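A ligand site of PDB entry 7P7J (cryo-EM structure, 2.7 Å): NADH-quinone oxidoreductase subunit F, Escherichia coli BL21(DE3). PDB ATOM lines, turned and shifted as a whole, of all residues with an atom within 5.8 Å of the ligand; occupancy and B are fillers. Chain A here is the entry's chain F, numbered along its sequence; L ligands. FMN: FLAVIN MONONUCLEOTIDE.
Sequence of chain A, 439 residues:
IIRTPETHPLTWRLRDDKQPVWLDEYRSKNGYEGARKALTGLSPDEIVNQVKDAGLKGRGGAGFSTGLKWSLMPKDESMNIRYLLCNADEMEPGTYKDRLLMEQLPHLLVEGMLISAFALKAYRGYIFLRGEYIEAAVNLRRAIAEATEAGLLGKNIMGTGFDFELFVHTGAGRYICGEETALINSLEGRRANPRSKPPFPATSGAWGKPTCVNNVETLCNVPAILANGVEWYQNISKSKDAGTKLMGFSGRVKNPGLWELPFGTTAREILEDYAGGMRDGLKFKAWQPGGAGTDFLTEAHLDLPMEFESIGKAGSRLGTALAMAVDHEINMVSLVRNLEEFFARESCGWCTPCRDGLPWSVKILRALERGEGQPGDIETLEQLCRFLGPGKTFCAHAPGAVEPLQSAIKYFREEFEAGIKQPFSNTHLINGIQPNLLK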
ATOM      1  N   LYS A  57       1.040  -7.778  17.593  1.00  0.00           N
ATOM      2  CA  LYS A  57       0.400  -6.485  17.647  1.00  0.00           C
ATOM      3  C   LYS A  57       1.309  -5.428  17.022  1.00  0.00           C
ATOM      4  O   LYS A  57       2.488  -5.661  16.760  1.00  0.00           O
ATOM      5  CB  LYS A  57       0.050  -6.107  19.089  1.00  0.00           C
ATOM      6  CG  LYS A  57      -0.972  -7.018  19.726  1.00  0.00           C
ATOM      7  CD  LYS A  57      -1.406  -6.512  21.084  1.00  0.00           C
ATOM      8  CE  LYS A  57      -2.313  -7.500  21.782  1.00  0.00           C
ATOM      9  NZ  LYS A  57      -1.637  -8.808  22.009  1.00  0.00           N
ATOM     10  N   GLY A  58       0.735  -4.261  16.764  1.00  0.00           N
ATOM     11  CA  GLY A  58       1.497  -3.188  16.151  1.00  0.00           C
ATOM     12  C   GLY A  58       2.521  -2.604  17.117  1.00  0.00           C
ATOM     13  O   GLY A  58       2.361  -2.628  18.329  1.00  0.00           O
ATOM     14  N   ARG A  59       3.596  -2.080  16.537  1.00  0.00           N
ATOM     15  CA  ARG A  59       4.686  -1.504  17.306  1.00  0.00           C
ATOM     16  C   ARG A  59       4.803   0.006  17.122  1.00  0.00           C
ATOM     17  O   ARG A  59       5.708   0.615  17.702  1.00  0.00           O
ATOM     18  CB  ARG A  59       6.011  -2.170  16.928  1.00  0.00           C
ATOM     19  CG  ARG A  59       5.961  -3.687  16.951  1.00  0.00           C
ATOM     20  CD  ARG A  59       5.666  -4.206  18.343  1.00  0.00           C
ATOM     21  NE  ARG A  59       6.272  -5.519  18.571  1.00  0.00           N
ATOM     22  CZ  ARG A  59       5.580  -6.642  18.697  1.00  0.00           C
ATOM     23  NH1 ARG A  59       4.258  -6.656  18.637  1.00  0.00           N
ATOM     24  NH2 ARG A  59       6.233  -7.787  18.896  1.00  0.00           N
ATOM     25  N   GLY A  60       3.923   0.624  16.341  1.00  0.00           N
ATOM     26  CA  GLY A  60       3.981   2.064  16.148  1.00  0.00           C
ATOM     27  C   GLY A  60       3.491   2.865  17.324  1.00  0.00           C
ATOM     28  O   GLY A  60       3.880   4.028  17.473  1.00  0.00           O
ATOM     29  N   GLY A  61       2.658   2.276  18.180  1.00  0.00           N
ATOM     30  CA  GLY A  61       2.150   2.970  19.334  1.00  0.00           C
ATOM     31  C   GLY A  61       0.696   2.693  19.617  1.00  0.00           C
ATOM     32  O   GLY A  61       0.235   2.807  20.757  1.00  0.00           O
ATOM     33  N   ALA A  62      -0.062   2.325  18.579  1.00  0.00           N
ATOM     34  CA  ALA A  62      -1.475   2.010  18.754  1.00  0.00           C
ATOM     35  C   ALA A  62      -1.675   0.637  19.378  1.00  0.00           C
ATOM     36  O   ALA A  62      -2.643   0.447  20.131  1.00  0.00           O
ATOM     37  CB  ALA A  62      -2.206   2.094  17.424  1.00  0.00           C
ATOM     38  N   GLY A  63      -0.800  -0.310  19.091  1.00  0.00           N
ATOM     39  CA  GLY A  63      -0.897  -1.639  19.662  1.00  0.00           C
ATOM     40  C   GLY A  63      -1.959  -2.529  19.042  1.00  0.00           C
ATOM     41  O   GLY A  63      -2.271  -3.573  19.610  1.00  0.00           O
ATOM     42  N   PHE A  64      -2.512  -2.140  17.895  1.00  0.00           N
ATOM     43  CA  PHE A  64      -3.518  -2.958  17.235  1.00  0.00           C
ATOM     44  C   PHE A  64      -2.871  -4.196  16.618  1.00  0.00           C
ATOM     45  O   PHE A  64      -1.721  -4.163  16.150  1.00  0.00           O
ATOM     46  CB  PHE A  64      -4.236  -2.151  16.162  1.00  0.00           C
ATOM     47  CG  PHE A  64      -5.465  -2.815  15.618  1.00  0.00           C
ATOM     48  CD1 PHE A  64      -6.586  -2.986  16.414  1.00  0.00           C
ATOM     49  CD2 PHE A  64      -5.509  -3.253  14.307  1.00  0.00           C
ATOM     50  CE1 PHE A  64      -7.718  -3.591  15.914  1.00  0.00           C
ATOM     51  CE2 PHE A  64      -6.629  -3.865  13.803  1.00  0.00           C
ATOM     52  CZ  PHE A  64      -7.737  -4.031  14.604  1.00  0.00           C
ATOM     53  N   THR A  66      -1.829  -7.070  14.114  1.00  0.00           N
ATOM     54  CA  THR A  66      -1.528  -7.017  12.685  1.00  0.00           C
ATOM     55  C   THR A  66      -2.450  -7.944  11.893  1.00  0.00           C
ATOM     56  O   THR A  66      -2.822  -7.625  10.757  1.00  0.00           O
ATOM     57  CB  THR A  66      -0.069  -7.388  12.448  1.00  0.00           C
ATOM     58  OG1 THR A  66       0.739  -6.818  13.482  1.00  0.00           O
ATOM     59  CG2 THR A  66       0.402  -6.853  11.106  1.00  0.00           C
ATOM     60  N   LYS A  69      -5.853  -6.274  11.343  1.00  0.00           N
ATOM     61  CA  LYS A  69      -5.749  -5.234  10.318  1.00  0.00           C
ATOM     62  C   LYS A  69      -5.612  -5.847   8.933  1.00  0.00           C
ATOM     63  O   LYS A  69      -6.184  -5.328   7.957  1.00  0.00           O
ATOM     64  CB  LYS A  69      -4.560  -4.320  10.620  1.00  0.00           C
ATOM     65  CG  LYS A  69      -4.400  -3.161   9.669  1.00  0.00           C
ATOM     66  CD  LYS A  69      -3.047  -2.494   9.807  1.00  0.00           C
ATOM     67  CE  LYS A  69      -2.918  -1.804  11.141  1.00  0.00           C
ATOM     68  NZ  LYS A  69      -1.661  -1.014  11.227  1.00  0.00           N
ATOM     69  N   ASN A  87       5.845   2.459   7.744  1.00  0.00           N
ATOM     70  CA  ASN A  87       5.938   3.723   8.456  1.00  0.00           C
ATOM     71  C   ASN A  87       7.325   3.837   9.080  1.00  0.00           C
ATOM     72  O   ASN A  87       7.526   3.628  10.280  1.00  0.00           O
ATOM     73  CB  ASN A  87       4.843   3.819   9.508  1.00  0.00           C
ATOM     74  CG  ASN A  87       4.575   5.239   9.960  1.00  0.00           C
ATOM     75  OD1 ASN A  87       5.435   6.104   9.885  1.00  0.00           O
ATOM     76  ND2 ASN A  87       3.351   5.490  10.416  1.00  0.00           N
ATOM     77  N   ALA A  88       8.322   4.136   8.238  1.00  0.00           N
ATOM     78  CA  ALA A  88       9.672   4.383   8.696  1.00  0.00           C
ATOM     79  C   ALA A  88       9.897   5.842   9.087  1.00  0.00           C
ATOM     80  O   ALA A  88      11.042   6.291   9.117  1.00  0.00           O
ATOM     81  CB  ALA A  88      10.668   3.974   7.610  1.00  0.00           C
ATOM     82  N   ASP A  89       8.818   6.583   9.346  1.00  0.00           N
ATOM     83  CA  ASP A  89       8.940   7.996   9.675  1.00  0.00           C
ATOM     84  C   ASP A  89       9.651   8.200  10.996  1.00  0.00           C
ATOM     85  O   ASP A  89      10.637   8.950  11.071  1.00  0.00           O
ATOM     86  CB  ASP A  89       7.560   8.640   9.691  1.00  0.00           C
ATOM     87  CG  ASP A  89       7.576  10.087   9.217  1.00  0.00           C
ATOM     88  OD1 ASP A  89       8.568  10.485   8.575  1.00  0.00           O
ATOM     89  OD2 ASP A  89       6.598  10.816   9.473  1.00  0.00           O
ATOM     90  N   GLU A  90       9.189   7.517  12.051  1.00  0.00           N
ATOM     91  CA  GLU A  90       9.768   7.567  13.399  1.00  0.00           C
ATOM     92  C   GLU A  90       9.913   9.005  13.908  1.00  0.00           C
ATOM     93  O   GLU A  90      10.935   9.385  14.481  1.00  0.00           O
ATOM     94  CB  GLU A  90      11.100   6.825  13.471  1.00  0.00           C
ATOM     95  CG  GLU A  90      11.295   6.092  14.776  1.00  0.00           C
ATOM     96  CD  GLU A  90      12.716   5.659  15.007  1.00  0.00           C
ATOM     97  OE1 GLU A  90      13.641   6.305  14.450  1.00  0.00           O
ATOM     98  OE2 GLU A  90      12.925   4.676  15.743  1.00  0.00           O
ATOM     99  N   MET A  91       8.887   9.809  13.659  1.00  0.00           N
ATOM    100  CA  MET A  91       8.927  11.224  13.992  1.00  0.00           C
ATOM    101  C   MET A  91       8.585  11.518  15.453  1.00  0.00           C
ATOM    102  O   MET A  91       8.719  12.660  15.874  1.00  0.00           O
ATOM    103  CB  MET A  91       7.978  11.994  13.068  1.00  0.00           C
ATOM    104  CG  MET A  91       8.536  12.351  11.687  1.00  0.00           C
ATOM    105  SD  MET A  91      10.089  13.255  11.574  1.00  0.00           S
ATOM    106  CE  MET A  91       9.955  14.443  12.918  1.00  0.00           C
ATOM    107  N   GLU A  92       8.141  10.518  16.207  1.00  0.00           N
ATOM    108  CA  GLU A  92       7.851  10.723  17.618  1.00  0.00           C
ATOM    109  C   GLU A  92       9.142  10.964  18.386  1.00  0.00           C
ATOM    110  O   GLU A  92      10.117  10.227  18.202  1.00  0.00           O
ATOM    111  CB  GLU A  92       7.119   9.505  18.187  1.00  0.00           C
ATOM    112  CG  GLU A  92       6.867   9.575  19.684  1.00  0.00           C
ATOM    113  CD  GLU A  92       5.476  10.058  20.027  1.00  0.00           C
ATOM    114  OE1 GLU A  92       5.090  11.149  19.574  1.00  0.00           O
ATOM    115  OE2 GLU A  92       4.755   9.345  20.757  1.00  0.00           O
ATOM    116  N   ASP A  98      13.687   2.343  15.041  1.00  0.00           N
ATOM    117  CA  ASP A  98      13.675   2.093  13.604  1.00  0.00           C
ATOM    118  C   ASP A  98      14.976   2.520  12.949  1.00  0.00           C
ATOM    119  O   ASP A  98      15.400   1.900  11.974  1.00  0.00           O
ATOM    120  CB  ASP A  98      12.489   2.797  12.965  1.00  0.00           C
ATOM    121  CG  ASP A  98      11.170   2.402  13.577  1.00  0.00           C
ATOM    122  OD1 ASP A  98      11.075   1.279  14.118  1.00  0.00           O
ATOM    123  OD2 ASP A  98      10.209   3.196  13.517  1.00  0.00           O
ATOM    124  N   TYR A 175       6.066  15.879  11.452  1.00  0.00           N
ATOM    125  CA  TYR A 175       5.743  14.837  12.423  1.00  0.00           C
ATOM    126  C   TYR A 175       4.411  14.179  12.129  1.00  0.00           C
ATOM    127  O   TYR A 175       4.243  12.976  12.400  1.00  0.00           O
ATOM    128  CB  TYR A 175       5.750  15.425  13.832  1.00  0.00           C
ATOM    129  CG  TYR A 175       5.070  14.567  14.886  1.00  0.00           C
ATOM    130  CD1 TYR A 175       5.613  13.363  15.293  1.00  0.00           C
ATOM    131  CD2 TYR A 175       3.883  14.984  15.461  1.00  0.00           C
ATOM    132  CE1 TYR A 175       5.002  12.590  16.239  1.00  0.00           C
ATOM    133  CE2 TYR A 175       3.258  14.208  16.425  1.00  0.00           C
ATOM    134  CZ  TYR A 175       3.825  13.012  16.806  1.00  0.00           C
ATOM    135  OH  TYR A 175       3.205  12.234  17.761  1.00  0.00           O
ATOM    136  N   ILE A 176       3.450  14.917  11.560  1.00  0.00           N
ATOM    137  CA  ILE A 176       2.118  14.387  11.330  1.00  0.00           C
ATOM    138  C   ILE A 176       2.114  13.340  10.221  1.00  0.00           C
ATOM    139  O   ILE A 176       1.162  12.571  10.100  1.00  0.00           O
ATOM    140  CB  ILE A 176       1.147  15.551  11.043  1.00  0.00           C
ATOM    141  CG1 ILE A 176      -0.315  15.126  11.180  1.00  0.00           C
ATOM    142  CG2 ILE A 176       1.393  16.122   9.667  1.00  0.00           C
ATOM    143  CD1 ILE A 176      -0.611  14.339  12.435  1.00  0.00           C
ATOM    144  N   CYS A 177       3.192  13.259   9.437  1.00  0.00           N
ATOM    145  CA  CYS A 177       3.304  12.252   8.386  1.00  0.00           C
ATOM    146  C   CYS A 177       3.384  10.832   8.937  1.00  0.00           C
ATOM    147  O   CYS A 177       3.189   9.879   8.179  1.00  0.00           O
ATOM    148  CB  CYS A 177       4.530  12.523   7.520  1.00  0.00           C
ATOM    149  SG  CYS A 177       4.562  14.152   6.785  1.00  0.00           S
ATOM    150  N   GLY A 178       3.682  10.662  10.222  1.00  0.00           N
ATOM    151  CA  GLY A 178       3.682   9.334  10.807  1.00  0.00           C
ATOM    152  C   GLY A 178       2.310   8.743  11.009  1.00  0.00           C
ATOM    153  O   GLY A 178       2.180   7.527  11.081  1.00  0.00           O
ATOM    154  N   GLU A 179       1.281   9.590  11.108  1.00  0.00           N
ATOM    155  CA  GLU A 179      -0.089   9.110  11.146  1.00  0.00           C
ATOM    156  C   GLU A 179      -0.426   8.414   9.835  1.00  0.00           C
ATOM    157  O   GLU A 179      -0.097   8.908   8.760  1.00  0.00           O
ATOM    158  CB  GLU A 179      -1.041  10.286  11.380  1.00  0.00           C
ATOM    159  CG  GLU A 179      -2.285   9.944  12.177  1.00  0.00           C
ATOM    160  CD  GLU A 179      -3.394   9.365  11.318  1.00  0.00           C
ATOM    161  OE1 GLU A 179      -3.382   9.600  10.103  1.00  0.00           O
ATOM    162  OE2 GLU A 179      -4.274   8.682  11.875  1.00  0.00           O
ATOM    163  N   GLU A 180      -1.076   7.244   9.940  1.00  0.00           N
ATOM    164  CA  GLU A 180      -1.161   6.313   8.810  1.00  0.00           C
ATOM    165  C   GLU A 180      -1.947   6.905   7.642  1.00  0.00           C
ATOM    166  O   GLU A 180      -1.507   6.803   6.486  1.00  0.00           O
ATOM    167  CB  GLU A 180      -1.783   4.995   9.257  1.00  0.00           C
ATOM    168  CG  GLU A 180      -2.957   5.135  10.207  1.00  0.00           C
ATOM    169  CD  GLU A 180      -3.703   3.837  10.384  1.00  0.00           C
ATOM    170  OE1 GLU A 180      -3.330   2.837   9.736  1.00  0.00           O
ATOM    171  OE2 GLU A 180      -4.673   3.810  11.177  1.00  0.00           O
ATOM    172  N   VAL A 213      -0.780  -0.140   6.198  1.00  0.00           N
ATOM    173  CA  VAL A 213       0.367   0.595   6.724  1.00  0.00           C
ATOM    174  C   VAL A 213       0.819  -0.091   8.007  1.00  0.00           C
ATOM    175  O   VAL A 213       0.012  -0.301   8.919  1.00  0.00           O
ATOM    176  CB  VAL A 213       0.023   2.067   6.980  1.00  0.00           C
ATOM    177  CG1 VAL A 213       1.252   2.833   7.432  1.00  0.00           C
ATOM    178  CG2 VAL A 213      -0.564   2.704   5.736  1.00  0.00           C
ATOM    179  N   ASN A 214       2.101  -0.424   8.075  1.00  0.00           N
ATOM    180  CA  ASN A 214       2.652  -1.111   9.234  1.00  0.00           C
ATOM    181  C   ASN A 214       3.990  -0.512   9.608  1.00  0.00           C
ATOM    182  O   ASN A 214       4.699   0.045   8.770  1.00  0.00           O
ATOM    183  CB  ASN A 214       2.799  -2.619   8.981  1.00  0.00           C
ATOM    184  CG  ASN A 214       1.462  -3.328   8.922  1.00  0.00           C
ATOM    185  OD1 ASN A 214       1.115  -3.921   7.901  1.00  0.00           O
ATOM    186  ND2 ASN A 214       0.718  -3.271  10.017  1.00  0.00           N
ATOM    187  N   ASN A 215       4.334  -0.628  10.889  1.00  0.00           N
ATOM    188  CA  ASN A 215       5.594  -0.097  11.397  1.00  0.00           C
ATOM    189  C   ASN A 215       6.766  -0.953  10.931  1.00  0.00           C
ATOM    190  O   ASN A 215       6.598  -2.077  10.439  1.00  0.00           O
ATOM    191  CB  ASN A 215       5.545  -0.028  12.929  1.00  0.00           C
ATOM    192  CG  ASN A 215       6.619   0.877  13.504  1.00  0.00           C
ATOM    193  OD1 ASN A 215       7.247   1.644  12.778  1.00  0.00           O
ATOM    194  ND2 ASN A 215       6.853   0.767  14.795  1.00  0.00           N
ATOM    195  N   VAL A 216       7.976  -0.400  11.066  1.00  0.00           N
ATOM    196  CA  VAL A 216       9.200  -1.134  10.740  1.00  0.00           C
ATOM    197  C   VAL A 216       9.347  -2.355  11.625  1.00  0.00           C
ATOM    198  O   VAL A 216       9.702  -3.445  11.160  1.00  0.00           O
ATOM    199  CB  VAL A 216      10.422  -0.219  10.861  1.00  0.00           C
ATOM    200  CG1 VAL A 216      11.655  -0.882  10.271  1.00  0.00           C
ATOM    201  CG2 VAL A 216      10.151   1.101  10.196  1.00  0.00           C
ATOM    202  N   THR A 218       7.099  -4.145  13.310  1.00  0.00           N
ATOM    203  CA  THR A 218       6.130  -5.197  13.024  1.00  0.00           C
ATOM    204  C   THR A 218       6.573  -6.040  11.824  1.00  0.00           C
ATOM    205  O   THR A 218       6.570  -7.284  11.866  1.00  0.00           O
ATOM    206  CB  THR A 218       4.757  -4.585  12.773  1.00  0.00           C
ATOM    207  OG1 THR A 218       4.364  -3.818  13.917  1.00  0.00           O
ATOM    208  CG2 THR A 218       3.726  -5.658  12.520  1.00  0.00           C
ATOM    209  N   CYS A 395      -7.892  13.757  14.555  1.00  0.00           N
ATOM    210  CA  CYS A 395      -6.975  12.619  14.632  1.00  0.00           C
ATOM    211  C   CYS A 395      -6.423  12.490  16.047  1.00  0.00           C
ATOM    212  O   CYS A 395      -6.864  13.188  16.954  1.00  0.00           O
ATOM    213  CB  CYS A 395      -5.858  12.753  13.600  1.00  0.00           C
ATOM    214  SG  CYS A 395      -4.374  13.595  14.172  1.00  0.00           S
ATOM    215  N   ALA A 396      -5.460  11.593  16.234  1.00  0.00           N
ATOM    216  CA  ALA A 396      -4.964  11.252  17.559  1.00  0.00           C
ATOM    217  C   ALA A 396      -3.736  12.054  17.965  1.00  0.00           C
ATOM    218  O   ALA A 396      -3.122  11.731  18.982  1.00  0.00           O
ATOM    219  CB  ALA A 396      -4.649   9.757  17.635  1.00  0.00           C
ATOM    220  N   HIS A 397      -3.368  13.073  17.200  1.00  0.00           N
ATOM    221  CA  HIS A 397      -2.201  13.885  17.547  1.00  0.00           C
ATOM    222  C   HIS A 397      -2.459  14.716  18.800  1.00  0.00           C
ATOM    223  O   HIS A 397      -1.588  14.854  19.664  1.00  0.00           O
ATOM    224  CB  HIS A 397      -1.809  14.780  16.378  1.00  0.00           C
ATOM    225  CG  HIS A 397      -0.901  15.903  16.750  1.00  0.00           C
ATOM    226  ND1 HIS A 397       0.463  15.744  16.899  1.00  0.00           N
ATOM    227  CD2 HIS A 397      -1.151  17.217  16.976  1.00  0.00           C
ATOM    228  CE1 HIS A 397       1.001  16.906  17.219  1.00  0.00           C
ATOM    229  NE2 HIS A 397       0.051  17.811  17.270  1.00  0.00           N
HETATM  230  N1  FMN L   1       3.684   5.131  13.733  1.00  0.00           N
HETATM  231  C2  FMN L   1       4.970   4.857  13.340  1.00  0.00           C
HETATM  232  O2  FMN L   1       5.291   3.699  13.102  1.00  0.00           O
HETATM  233  N3  FMN L   1       5.886   5.873  13.212  1.00  0.00           N
HETATM  234  C4  FMN L   1       5.521   7.174  13.476  1.00  0.00           C
HETATM  235  O4  FMN L   1       6.322   8.084  13.368  1.00  0.00           O
HETATM  236  C4A FMN L   1       4.217   7.446  13.872  1.00  0.00           C
HETATM  237  N5  FMN L   1       3.846   8.738  14.136  1.00  0.00           N
HETATM  238  C5A FMN L   1       2.552   9.017  14.523  1.00  0.00           C
HETATM  239  C6  FMN L   1       2.191  10.325  14.787  1.00  0.00           C
HETATM  240  C7  FMN L   1       0.897  10.616  15.182  1.00  0.00           C
HETATM  241  C7M FMN L   1       0.522  12.037  15.461  1.00  0.00           C
HETATM  242  C8  FMN L   1      -0.035   9.597  15.314  1.00  0.00           C
HETATM  243  C8M FMN L   1      -1.437   9.904  15.743  1.00  0.00           C
HETATM  244  C9  FMN L   1       0.325   8.289  15.051  1.00  0.00           C
HETATM  245  C9A FMN L   1       1.626   7.983  14.652  1.00  0.00           C
HETATM  246  N10 FMN L   1       2.004   6.676  14.385  1.00  0.00           N
HETATM  247  C10 FMN L   1       3.296   6.421  14.000  1.00  0.00           C
HETATM  248  C1' FMN L   1       1.039   5.537  14.503  1.00  0.00           C
HETATM  249  C2' FMN L   1       0.351   5.296  13.158  1.00  0.00           C
HETATM  250  O2' FMN L   1      -0.852   6.021  13.100  1.00  0.00           O
HETATM  251  C3' FMN L   1       0.040   3.820  12.915  1.00  0.00           C
HETATM  252  O3' FMN L   1      -0.672   3.293  14.012  1.00  0.00           O
HETATM  253  C4' FMN L   1       1.324   3.031  12.708  1.00  0.00           C
HETATM  254  O4' FMN L   1       2.218   3.771  11.907  1.00  0.00           O
HETATM  255  C5' FMN L   1       1.087   1.678  12.055  1.00  0.00           C
HETATM  256  O5' FMN L   1       0.457   0.824  12.982  1.00  0.00           O
HETATM  257  P   FMN L   1       1.220  -0.506  13.472  1.00  0.00           P
HETATM  258  O1P FMN L   1       1.853  -0.210  14.806  1.00  0.00           O
HETATM  259  O2P FMN L   1       0.224  -1.639  13.584  1.00  0.00           O
HETATM  260  O3P FMN L   1       2.300  -0.869  12.497  1.00  0.00           O
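ND2 of Asn 87 is in hydrogen-bond range of O4' of the ligand (2.5 Å).
The backbone NH (N) of Asn 215 is in hydrogen-bond range of an oxygen (O3P) of the ligand (2.6 Å).
The side-chain amide oxygen of Asn 215 lies close to an oxygen (O2) of the ligand (2.9 Å).
The backbone NH (N) of Gly 60 sits at hydrogen-bond distance from an oxygen (O1P) of the ligand, 2.7 Å away.
The side-chain amino group (NZ) of Lys 69 lies within salt-bridge range of an oxygen (O2P) of the ligand (3.1 Å).
The backbone NH (N) of Arg 59 lies within hydrogen-bond range of an oxygen (O1P) of the ligand (3.1 Å).
An oxygen (O4) of the ligand lies within hydrogen-bond range of the backbone NH (N) of Met 91 (3.1 Å).
An oxygen (O4) of the ligand sits at hydrogen-bond distance from the backbone NH of Glu 90 (3.2 Å).
N of Glu 180 lies within hydrogen-bond range of O2' of the ligand, 3.4 Å away.
The backbone carbonyl oxygen (O) of Gly 178 sits at hydrogen-bond distance from the side-chain amide nitrogen (ND2) of Asn 87, 2.4 Å away.
The side-chain amide oxygen (OD1) of Asn 87 sits close to the backbone NH (N) of Asp 89 (3.5 Å).
The backbone NH (N) of Gly 60 lies close to the side-chain amide nitrogen (ND2) of Asn 215.
The backbone carbonyl oxygen (O) of Arg 59 lies within hydrogen-bond range of the side-chain amide nitrogen (ND2) of Asn 215.
The side-chain amide oxygen (OD1) of Asn 215 sits close to the side-chain carboxylate (OD2) of Asp 98, at 3.4 Å.
The backbone NH of Arg 59 is in hydrogen-bond range of the side-chain hydroxyl of Thr 218.
The backbone NH of Gly 58 is in hydrogen-bond range of the backbone carbonyl oxygen of Phe 64, at 2.5 Å.
The side-chain carboxylate (OD2) of Asp 89 is in hydrogen-bond range of the backbone NH (N) of Gly 178 (3.0 Å).
A nitrogen (N10) of the ligand sits close to the backbone carbonyl oxygen (O) of Gly 178.
Gly 58 touches the ligand.
Ala 62 touches the ligand (CB to O3', 3.9 Å).
Asp 89 touches the ligand (CB to O4, 3.9 Å).
Tyr 175 touches the ligand (OH to C7M, 3.5 Å).
Ile 176 touches the ligand (CD1 to C7M, 3.97 Å).
Glu 179 touches the ligand.
O of Val 213 touches C5' of the ligand, at 3.9 Å.
Asn 214 touches the ligand.
OG1 of Thr 218 touches O3P of the ligand, 3.9 Å away.
CB of Ala 396 touches C8M of the ligand, at 3.7 Å.
His 397 touches the ligand (CB to C7M, 3.7 Å).
Hydrophobic or aromatic side chains within 4 Å of the ligand: Ala 62, Tyr 175, Ile 176, Ala 396 and His 397.
The nearest printed residue that does not touch the ligand is Phe 64 (4.1 Å).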
